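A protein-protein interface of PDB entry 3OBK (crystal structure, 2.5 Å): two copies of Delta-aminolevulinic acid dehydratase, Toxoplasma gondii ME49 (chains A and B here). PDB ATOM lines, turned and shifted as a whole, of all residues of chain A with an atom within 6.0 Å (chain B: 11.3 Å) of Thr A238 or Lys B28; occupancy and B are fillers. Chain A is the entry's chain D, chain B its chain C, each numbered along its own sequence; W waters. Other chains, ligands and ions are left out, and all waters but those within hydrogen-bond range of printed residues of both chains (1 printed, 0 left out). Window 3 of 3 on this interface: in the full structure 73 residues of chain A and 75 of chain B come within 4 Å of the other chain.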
ATOM      1  N   ILE A 156      16.248   0.784   0.337  1.00  0.00           N
ATOM      2  CA  ILE A 156      16.544   2.066  -0.294  1.00  0.00           C
ATOM      3  C   ILE A 156      15.403   3.014   0.066  1.00  0.00           C
ATOM      4  O   ILE A 156      14.315   2.901  -0.471  1.00  0.00           O
ATOM      5  CB  ILE A 156      16.652   1.946  -1.845  1.00  0.00           C
ATOM      6  CG1 ILE A 156      17.561   0.775  -2.249  1.00  0.00           C
ATOM      7  CG2 ILE A 156      17.147   3.244  -2.459  1.00  0.00           C
ATOM      8  CD1 ILE A 156      18.783   0.640  -1.447  1.00  0.00           C
ATOM      9  N   MET A 185      14.612   6.209 -10.133  1.00  0.00           N
ATOM     10  CA  MET A 185      13.363   5.509  -9.952  1.00  0.00           C
ATOM     11  C   MET A 185      12.843   5.512  -8.512  1.00  0.00           C
ATOM     12  O   MET A 185      12.142   4.573  -8.125  1.00  0.00           O
ATOM     13  CB  MET A 185      13.472   4.078 -10.494  1.00  0.00           C
ATOM     14  CG  MET A 185      13.552   4.025 -12.005  1.00  0.00           C
ATOM     15  SD  MET A 185      11.978   4.523 -12.747  1.00  0.00           S
ATOM     16  CE  MET A 185      11.016   3.007 -12.640  1.00  0.00           C
ATOM     17  N   ASP A 235      20.042  -6.493  -5.303  1.00  0.00           N
ATOM     18  CA  ASP A 235      19.554  -6.053  -6.624  1.00  0.00           C
ATOM     19  C   ASP A 235      18.738  -4.753  -6.506  1.00  0.00           C
ATOM     20  O   ASP A 235      18.581  -4.223  -5.411  1.00  0.00           O
ATOM     21  CB  ASP A 235      18.770  -7.182  -7.327  1.00  0.00           C
ATOM     22  CG  ASP A 235      17.550  -7.679  -6.520  1.00  0.00           C
ATOM     23  OD1 ASP A 235      16.767  -6.861  -5.984  1.00  0.00           O
ATOM     24  OD2 ASP A 235      17.367  -8.921  -6.457  1.00  0.00           O
ATOM     25  N   LYS A 236      18.246  -4.244  -7.640  1.00  0.00           N
ATOM     26  CA  LYS A 236      17.502  -2.986  -7.675  1.00  0.00           C
ATOM     27  C   LYS A 236      16.019  -3.196  -7.933  1.00  0.00           C
ATOM     28  O   LYS A 236      15.302  -2.281  -8.332  1.00  0.00           O
ATOM     29  CB  LYS A 236      18.088  -2.054  -8.733  1.00  0.00           C
ATOM     30  CG  LYS A 236      19.590  -1.840  -8.572  1.00  0.00           C
ATOM     31  CD  LYS A 236      20.044  -0.663  -9.383  1.00  0.00           C
ATOM     32  CE  LYS A 236      21.499  -0.328  -9.123  1.00  0.00           C
ATOM     33  NZ  LYS A 236      21.974   0.771 -10.027  1.00  0.00           N
ATOM     34  N   LYS A 237      15.549  -4.394  -7.646  1.00  0.00           N
ATOM     35  CA  LYS A 237      14.194  -4.771  -7.973  1.00  0.00           C
ATOM     36  C   LYS A 237      13.116  -4.089  -7.109  1.00  0.00           C
ATOM     37  O   LYS A 237      11.959  -4.062  -7.500  1.00  0.00           O
ATOM     38  CB  LYS A 237      14.075  -6.294  -7.906  1.00  0.00           C
ATOM     39  CG  LYS A 237      14.937  -6.999  -8.938  1.00  0.00           C
ATOM     40  CD  LYS A 237      14.681  -8.515  -8.951  1.00  0.00           C
ATOM     41  CE  LYS A 237      15.589  -9.210  -9.963  1.00  0.00           C
ATOM     42  NZ  LYS A 237      15.426 -10.685  -9.995  1.00  0.00           N
ATOM     43  N   THR A 238      13.495  -3.530  -5.969  1.00  0.00           N
ATOM     44  CA  THR A 238      12.589  -2.708  -5.150  1.00  0.00           C
ATOM     45  C   THR A 238      12.424  -1.247  -5.662  1.00  0.00           C
ATOM     46  O   THR A 238      11.655  -0.441  -5.095  1.00  0.00           O
ATOM     47  CB  THR A 238      13.034  -2.680  -3.654  1.00  0.00           C
ATOM     48  OG1 THR A 238      14.370  -2.179  -3.566  1.00  0.00           O
ATOM     49  CG2 THR A 238      12.936  -4.081  -2.999  1.00  0.00           C
ATOM     50  N   TYR A 239      13.142  -0.872  -6.713  1.00  0.00           N
ATOM     51  CA  TYR A 239      12.851   0.427  -7.317  1.00  0.00           C
ATOM     52  C   TYR A 239      12.754   0.402  -8.844  1.00  0.00           C
ATOM     53  O   TYR A 239      11.828   0.967  -9.406  1.00  0.00           O
ATOM     54  CB  TYR A 239      13.787   1.533  -6.799  1.00  0.00           C
ATOM     55  CG  TYR A 239      15.280   1.221  -6.741  1.00  0.00           C
ATOM     56  CD1 TYR A 239      15.831   0.465  -5.674  1.00  0.00           C
ATOM     57  CD2 TYR A 239      16.151   1.737  -7.694  1.00  0.00           C
ATOM     58  CE1 TYR A 239      17.202   0.216  -5.591  1.00  0.00           C
ATOM     59  CE2 TYR A 239      17.528   1.487  -7.620  1.00  0.00           C
ATOM     60  CZ  TYR A 239      18.044   0.731  -6.558  1.00  0.00           C
ATOM     61  OH  TYR A 239      19.405   0.483  -6.487  1.00  0.00           O
ATOM     62  N   GLN A 240      13.689  -0.244  -9.507  1.00  0.00           N
ATOM     63  CA  GLN A 240      13.582  -0.444 -10.948  1.00  0.00           C
ATOM     64  C   GLN A 240      12.447  -1.440 -11.223  1.00  0.00           C
ATOM     65  O   GLN A 240      12.115  -2.256 -10.388  1.00  0.00           O
ATOM     66  CB  GLN A 240      14.933  -0.891 -11.531  1.00  0.00           C
ATOM     67  CG  GLN A 240      16.070   0.133 -11.245  1.00  0.00           C
ATOM     68  CD  GLN A 240      17.405  -0.210 -11.863  1.00  0.00           C
ATOM     69  OE1 GLN A 240      17.646  -1.341 -12.269  1.00  0.00           O
ATOM     70  NE2 GLN A 240      18.282   0.768 -11.926  1.00  0.00           N
ATOM     71  N   ARG B  22       2.619   5.642  -4.360  1.00  0.00           N
ATOM     72  CA  ARG B  22       3.985   5.162  -4.401  1.00  0.00           C
ATOM     73  C   ARG B  22       4.026   3.847  -5.165  1.00  0.00           C
ATOM     74  O   ARG B  22       3.808   2.786  -4.585  1.00  0.00           O
ATOM     75  CB  ARG B  22       4.490   4.967  -2.987  1.00  0.00           C
ATOM     76  CG  ARG B  22       4.625   6.261  -2.247  1.00  0.00           C
ATOM     77  CD  ARG B  22       5.221   6.064  -0.869  1.00  0.00           C
ATOM     78  NE  ARG B  22       5.271   7.337  -0.140  1.00  0.00           N
ATOM     79  CZ  ARG B  22       6.359   8.071   0.077  1.00  0.00           C
ATOM     80  NH1 ARG B  22       7.552   7.692  -0.341  1.00  0.00           N
ATOM     81  NH2 ARG B  22       6.238   9.209   0.740  1.00  0.00           N
ATOM     82  N   PRO B  23       4.297   3.907  -6.477  1.00  0.00           N
ATOM     83  CA  PRO B  23       4.459   2.660  -7.277  1.00  0.00           C
ATOM     84  C   PRO B  23       5.465   1.657  -6.724  1.00  0.00           C
ATOM     85  O   PRO B  23       5.283   0.456  -6.947  1.00  0.00           O
ATOM     86  CB  PRO B  23       4.935   3.157  -8.636  1.00  0.00           C
ATOM     87  CG  PRO B  23       4.354   4.557  -8.743  1.00  0.00           C
ATOM     88  CD  PRO B  23       4.318   5.119  -7.328  1.00  0.00           C
ATOM     89  N   ARG B  24       6.509   2.131  -6.035  1.00  0.00           N
ATOM     90  CA  ARG B  24       7.457   1.232  -5.382  1.00  0.00           C
ATOM     91  C   ARG B  24       6.821   0.236  -4.383  1.00  0.00           C
ATOM     92  O   ARG B  24       7.377  -0.836  -4.154  1.00  0.00           O
ATOM     93  CB  ARG B  24       8.573   2.027  -4.668  1.00  0.00           C
ATOM     94  CG  ARG B  24       9.604   2.639  -5.612  1.00  0.00           C
ATOM     95  CD  ARG B  24      10.761   3.271  -4.853  1.00  0.00           C
ATOM     96  NE  ARG B  24      11.587   2.260  -4.176  1.00  0.00           N
ATOM     97  CZ  ARG B  24      12.377   2.486  -3.128  1.00  0.00           C
ATOM     98  NH1 ARG B  24      12.521   3.701  -2.618  1.00  0.00           N
ATOM     99  NH2 ARG B  24      13.040   1.481  -2.595  1.00  0.00           N
ATOM    100  N   ARG B  25       5.681   0.569  -3.788  1.00  0.00           N
ATOM    101  CA  ARG B  25       5.062  -0.375  -2.860  1.00  0.00           C
ATOM    102  C   ARG B  25       4.801  -1.710  -3.554  1.00  0.00           C
ATOM    103  O   ARG B  25       4.977  -2.803  -2.947  1.00  0.00           O
ATOM    104  CB  ARG B  25       3.780   0.175  -2.253  1.00  0.00           C
ATOM    105  CG  ARG B  25       4.041   1.176  -1.157  1.00  0.00           C
ATOM    106  CD  ARG B  25       2.796   1.585  -0.404  1.00  0.00           C
ATOM    107  NE  ARG B  25       1.988   2.566  -1.148  1.00  0.00           N
ATOM    108  CZ  ARG B  25       1.806   3.851  -0.813  1.00  0.00           C
ATOM    109  NH1 ARG B  25       1.038   4.611  -1.580  1.00  0.00           N
ATOM    110  NH2 ARG B  25       2.392   4.403   0.251  1.00  0.00           N
ATOM    111  N   ASN B  26       4.412  -1.633  -4.830  1.00  0.00           N
ATOM    112  CA  ASN B  26       4.230  -2.850  -5.620  1.00  0.00           C
ATOM    113  C   ASN B  26       5.565  -3.538  -6.095  1.00  0.00           C
ATOM    114  O   ASN B  26       5.521  -4.531  -6.846  1.00  0.00           O
ATOM    115  CB  ASN B  26       3.191  -2.617  -6.750  1.00  0.00           C
ATOM    116  CG  ASN B  26       1.756  -2.350  -6.198  1.00  0.00           C
ATOM    117  OD1 ASN B  26       1.433  -2.673  -5.029  1.00  0.00           O
ATOM    118  ND2 ASN B  26       0.911  -1.725  -7.022  1.00  0.00           N
ATOM    119  N   ARG B  27       6.716  -3.045  -5.606  1.00  0.00           N
ATOM    120  CA  ARG B  27       8.058  -3.639  -5.867  1.00  0.00           C
ATOM    121  C   ARG B  27       8.806  -4.101  -4.607  1.00  0.00           C
ATOM    122  O   ARG B  27       9.946  -4.521  -4.690  1.00  0.00           O
ATOM    123  CB  ARG B  27       8.961  -2.633  -6.589  1.00  0.00           C
ATOM    124  CG  ARG B  27       8.263  -1.895  -7.706  1.00  0.00           C
ATOM    125  CD  ARG B  27       9.210  -1.267  -8.729  1.00  0.00           C
ATOM    126  NE  ARG B  27       8.356  -0.571  -9.676  1.00  0.00           N
ATOM    127  CZ  ARG B  27       8.271   0.748  -9.814  1.00  0.00           C
ATOM    128  NH1 ARG B  27       9.069   1.576  -9.123  1.00  0.00           N
ATOM    129  NH2 ARG B  27       7.394   1.247 -10.685  1.00  0.00           N
ATOM    130  N   LYS B  28       8.119  -4.043  -3.473  1.00  0.00           N
ATOM    131  CA  LYS B  28       8.663  -4.134  -2.110  1.00  0.00           C
ATOM    132  C   LYS B  28       9.473  -5.400  -1.808  1.00  0.00           C
ATOM    133  O   LYS B  28      10.454  -5.370  -1.094  1.00  0.00           O
ATOM    134  CB  LYS B  28       7.464  -4.125  -1.142  1.00  0.00           C
ATOM    135  CG  LYS B  28       7.422  -3.018  -0.140  1.00  0.00           C
ATOM    136  CD  LYS B  28       5.956  -2.630   0.234  1.00  0.00           C
ATOM    137  CE  LYS B  28       5.080  -3.743   0.786  1.00  0.00           C
ATOM    138  NZ  LYS B  28       4.086  -3.164   1.744  1.00  0.00           N
ATOM    139  N   ASN B  29       9.025  -6.528  -2.317  1.00  0.00           N
ATOM    140  CA  ASN B  29       9.693  -7.793  -2.079  1.00  0.00           C
ATOM    141  C   ASN B  29       9.179  -8.732  -3.141  1.00  0.00           C
ATOM    142  O   ASN B  29       8.195  -8.422  -3.819  1.00  0.00           O
ATOM    143  CB  ASN B  29       9.390  -8.325  -0.671  1.00  0.00           C
ATOM    144  CG  ASN B  29       7.870  -8.414  -0.369  1.00  0.00           C
ATOM    145  OD1 ASN B  29       7.108  -8.965  -1.143  1.00  0.00           O
ATOM    146  ND2 ASN B  29       7.452  -7.855   0.755  1.00  0.00           N
ATOM    147  N   ARG B  30       9.833  -9.879  -3.295  1.00  0.00           N
ATOM    148  CA  ARG B  30       9.495 -10.815  -4.367  1.00  0.00           C
ATOM    149  C   ARG B  30       8.023 -11.190  -4.344  1.00  0.00           C
ATOM    150  O   ARG B  30       7.366 -11.177  -5.390  1.00  0.00           O
ATOM    151  CB  ARG B  30      10.339 -12.080  -4.290  1.00  0.00           C
ATOM    152  CG  ARG B  30      10.004 -13.046  -5.401  1.00  0.00           C
ATOM    153  CD  ARG B  30      11.057 -14.096  -5.636  1.00  0.00           C
ATOM    154  NE  ARG B  30      10.745 -14.833  -6.868  1.00  0.00           N
ATOM    155  CZ  ARG B  30      10.859 -16.161  -7.041  1.00  0.00           C
ATOM    156  NH1 ARG B  30      11.280 -16.948  -6.071  1.00  0.00           N
ATOM    157  NH2 ARG B  30      10.527 -16.720  -8.211  1.00  0.00           N
ATOM    158  N   ALA B  31       7.516 -11.528  -3.161  1.00  0.00           N
ATOM    159  CA  ALA B  31       6.098 -11.905  -2.999  1.00  0.00           C
ATOM    160  C   ALA B  31       5.093 -10.879  -3.604  1.00  0.00           C
ATOM    161  O   ALA B  31       4.163 -11.267  -4.310  1.00  0.00           O
ATOM    162  CB  ALA B  31       5.785 -12.169  -1.526  1.00  0.00           C
ATOM    163  N   VAL B  32       5.287  -9.593  -3.341  1.00  0.00           N
ATOM    164  CA  VAL B  32       4.404  -8.574  -3.888  1.00  0.00           C
ATOM    165  C   VAL B  32       4.534  -8.533  -5.392  1.00  0.00           C
ATOM    166  O   VAL B  32       3.539  -8.512  -6.118  1.00  0.00           O
ATOM    167  CB  VAL B  32       4.719  -7.189  -3.338  1.00  0.00           C
ATOM    168  CG1 VAL B  32       3.893  -6.152  -4.024  1.00  0.00           C
ATOM    169  CG2 VAL B  32       4.448  -7.152  -1.865  1.00  0.00           C
ATOM    170  N   ARG B  33       5.768  -8.550  -5.862  1.00  0.00           N
ATOM    171  CA  ARG B  33       6.012  -8.487  -7.296  1.00  0.00           C
ATOM    172  C   ARG B  33       5.335  -9.631  -8.003  1.00  0.00           C
ATOM    173  O   ARG B  33       4.826  -9.460  -9.087  1.00  0.00           O
ATOM    174  CB  ARG B  33       7.510  -8.448  -7.592  1.00  0.00           C
ATOM    175  CG  ARG B  33       8.184  -7.185  -7.047  1.00  0.00           C
ATOM    176  CD  ARG B  33       9.540  -6.900  -7.722  1.00  0.00           C
ATOM    177  NE  ARG B  33      10.528  -7.912  -7.387  1.00  0.00           N
ATOM    178  CZ  ARG B  33      11.189  -7.957  -6.236  1.00  0.00           C
ATOM    179  NH1 ARG B  33      12.042  -8.953  -6.017  1.00  0.00           N
ATOM    180  NH2 ARG B  33      10.984  -7.022  -5.298  1.00  0.00           N
ATOM    181  N   GLN B  34       5.301 -10.793  -7.376  1.00  0.00           N
ATOM    182  CA  GLN B  34       4.636 -11.957  -7.958  1.00  0.00           C
ATOM    183  C   GLN B  34       3.102 -11.813  -7.978  1.00  0.00           C
ATOM    184  O   GLN B  34       2.430 -12.235  -8.932  1.00  0.00           O
ATOM    185  CB  GLN B  34       5.045 -13.237  -7.212  1.00  0.00           C
ATOM    186  CG  GLN B  34       6.487 -13.706  -7.481  1.00  0.00           C
ATOM    187  CD  GLN B  34       6.859 -15.005  -6.731  1.00  0.00           C
ATOM    188  OE1 GLN B  34       6.822 -15.082  -5.482  1.00  0.00           O
ATOM    189  NE2 GLN B  34       7.207 -16.039  -7.509  1.00  0.00           N
ATOM    190  N   LEU B  35       2.539 -11.244  -6.922  1.00  0.00           N
ATOM    191  CA  LEU B  35       1.117 -10.952  -6.931  1.00  0.00           C
ATOM    192  C   LEU B  35       0.731 -10.165  -8.191  1.00  0.00           C
ATOM    193  O   LEU B  35      -0.277 -10.469  -8.824  1.00  0.00           O
ATOM    194  CB  LEU B  35       0.689 -10.152  -5.696  1.00  0.00           C
ATOM    195  CG  LEU B  35       0.243 -10.891  -4.431  1.00  0.00           C
ATOM    196  CD1 LEU B  35      -0.397  -9.861  -3.506  1.00  0.00           C
ATOM    197  CD2 LEU B  35      -0.710 -12.099  -4.670  1.00  0.00           C
ATOM    198  N   VAL B  36       1.531  -9.168  -8.549  1.00  0.00           N
ATOM    199  CA  VAL B  36       1.148  -8.231  -9.597  1.00  0.00           C
ATOM    200  C   VAL B  36       1.828  -8.450 -10.952  1.00  0.00           C
ATOM    201  O   VAL B  36       1.777  -7.593 -11.801  1.00  0.00           O
ATOM    202  CB  VAL B  36       1.396  -6.776  -9.126  1.00  0.00           C
ATOM    203  CG1 VAL B  36       0.857  -6.616  -7.731  1.00  0.00           C
ATOM    204  CG2 VAL B  36       2.869  -6.405  -9.185  1.00  0.00           C
ATOM    205  N   GLN B  37       2.465  -9.592 -11.147  1.00  0.00           N
ATOM    206  CA  GLN B  37       3.299  -9.822 -12.318  1.00  0.00           C
ATOM    207  C   GLN B  37       2.362 -10.027 -13.498  1.00  0.00           C
ATOM    208  O   GLN B  37       1.546 -10.914 -13.473  1.00  0.00           O
ATOM    209  CB  GLN B  37       4.173 -11.052 -12.075  1.00  0.00           C
ATOM    210  CG  GLN B  37       5.001 -11.563 -13.275  1.00  0.00           C
ATOM    211  CD  GLN B  37       5.839 -12.793 -12.919  1.00  0.00           C
ATOM    212  OE1 GLN B  37       5.957 -13.139 -11.756  1.00  0.00           O
ATOM    213  NE2 GLN B  37       6.434 -13.450 -13.935  1.00  0.00           N
HETATM  214  O   HOH W   1       9.554   4.293  -8.521  1.00  0.00           O
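No position is printed for both chains.
Along chain B the printed residues that touch a printed residue of chain A span positions 24 to 33.
Along chain A the printed residues that touch a printed residue of chain B span positions 156 to 240.
Of the printed residues of chain B, Met A185 touches Arg B24 (3.8 Å).
No residue of chain B comes within 4 Å of Asp A235.
Of the printed residues of chain B, Thr A238 touches Arg B24, Arg B27 and Lys B28.
Of chain B, only Arg B24 and Arg B27 come within 4 Å of Tyr A239.
Of the printed residues of chain B, Gln A240 touches Arg B27.
Of the printed residues of chain A, Arg B24 touches Ile A156, Met A185, Thr A238 and Tyr A239.
The nearest residue of chain A that does not touch Lys B28 is Lys A237 (5.6 Å).
The nearest printed residue of chain A that does not touch Arg B24 is Gln A240 (6.3 Å).
O of Arg B27 sits at hydrogen-bond distance from NH2 of Arg B33 (2.8 Å).
O of Asn B29 lies close to NH2 of Arg B33.
The side-chain carboxylate (OD1) of Asp A235 lies within hydrogen-bond range of the backbone NH (N) of Lys A237 (3.2 Å).
Water W1 lies within hydrogen-bond range of O of Met A185 (2.6 Å) and NH1 of Arg B27 (2.8 Å).
NH2 of Arg B24 is in hydrogen-bond range of O of Ile A156, at 2.9 Å.
The backbone carbonyl oxygen of Thr A238 lies within hydrogen-bond range of the guanidinium group of Arg B24.
NH1 of Arg B27 is in hydrogen-bond range of O of Tyr A239 (2.8 Å).
O of Arg B27 sits close to O of Lys A237, 3.5 Å away.
Arg B24 touches Met A185 (CD to O, 3.8 Å).
CB of Lys A237 touches CZ of Arg B33, 3.7 Å away.
Thr A238 touches Arg B27 (CA to O, 3.2 Å).
Thr A238 touches Lys B28.
CB of Tyr A239 touches NE of Arg B24, at 3.5 Å.
Arg B27 touches Gln A240.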
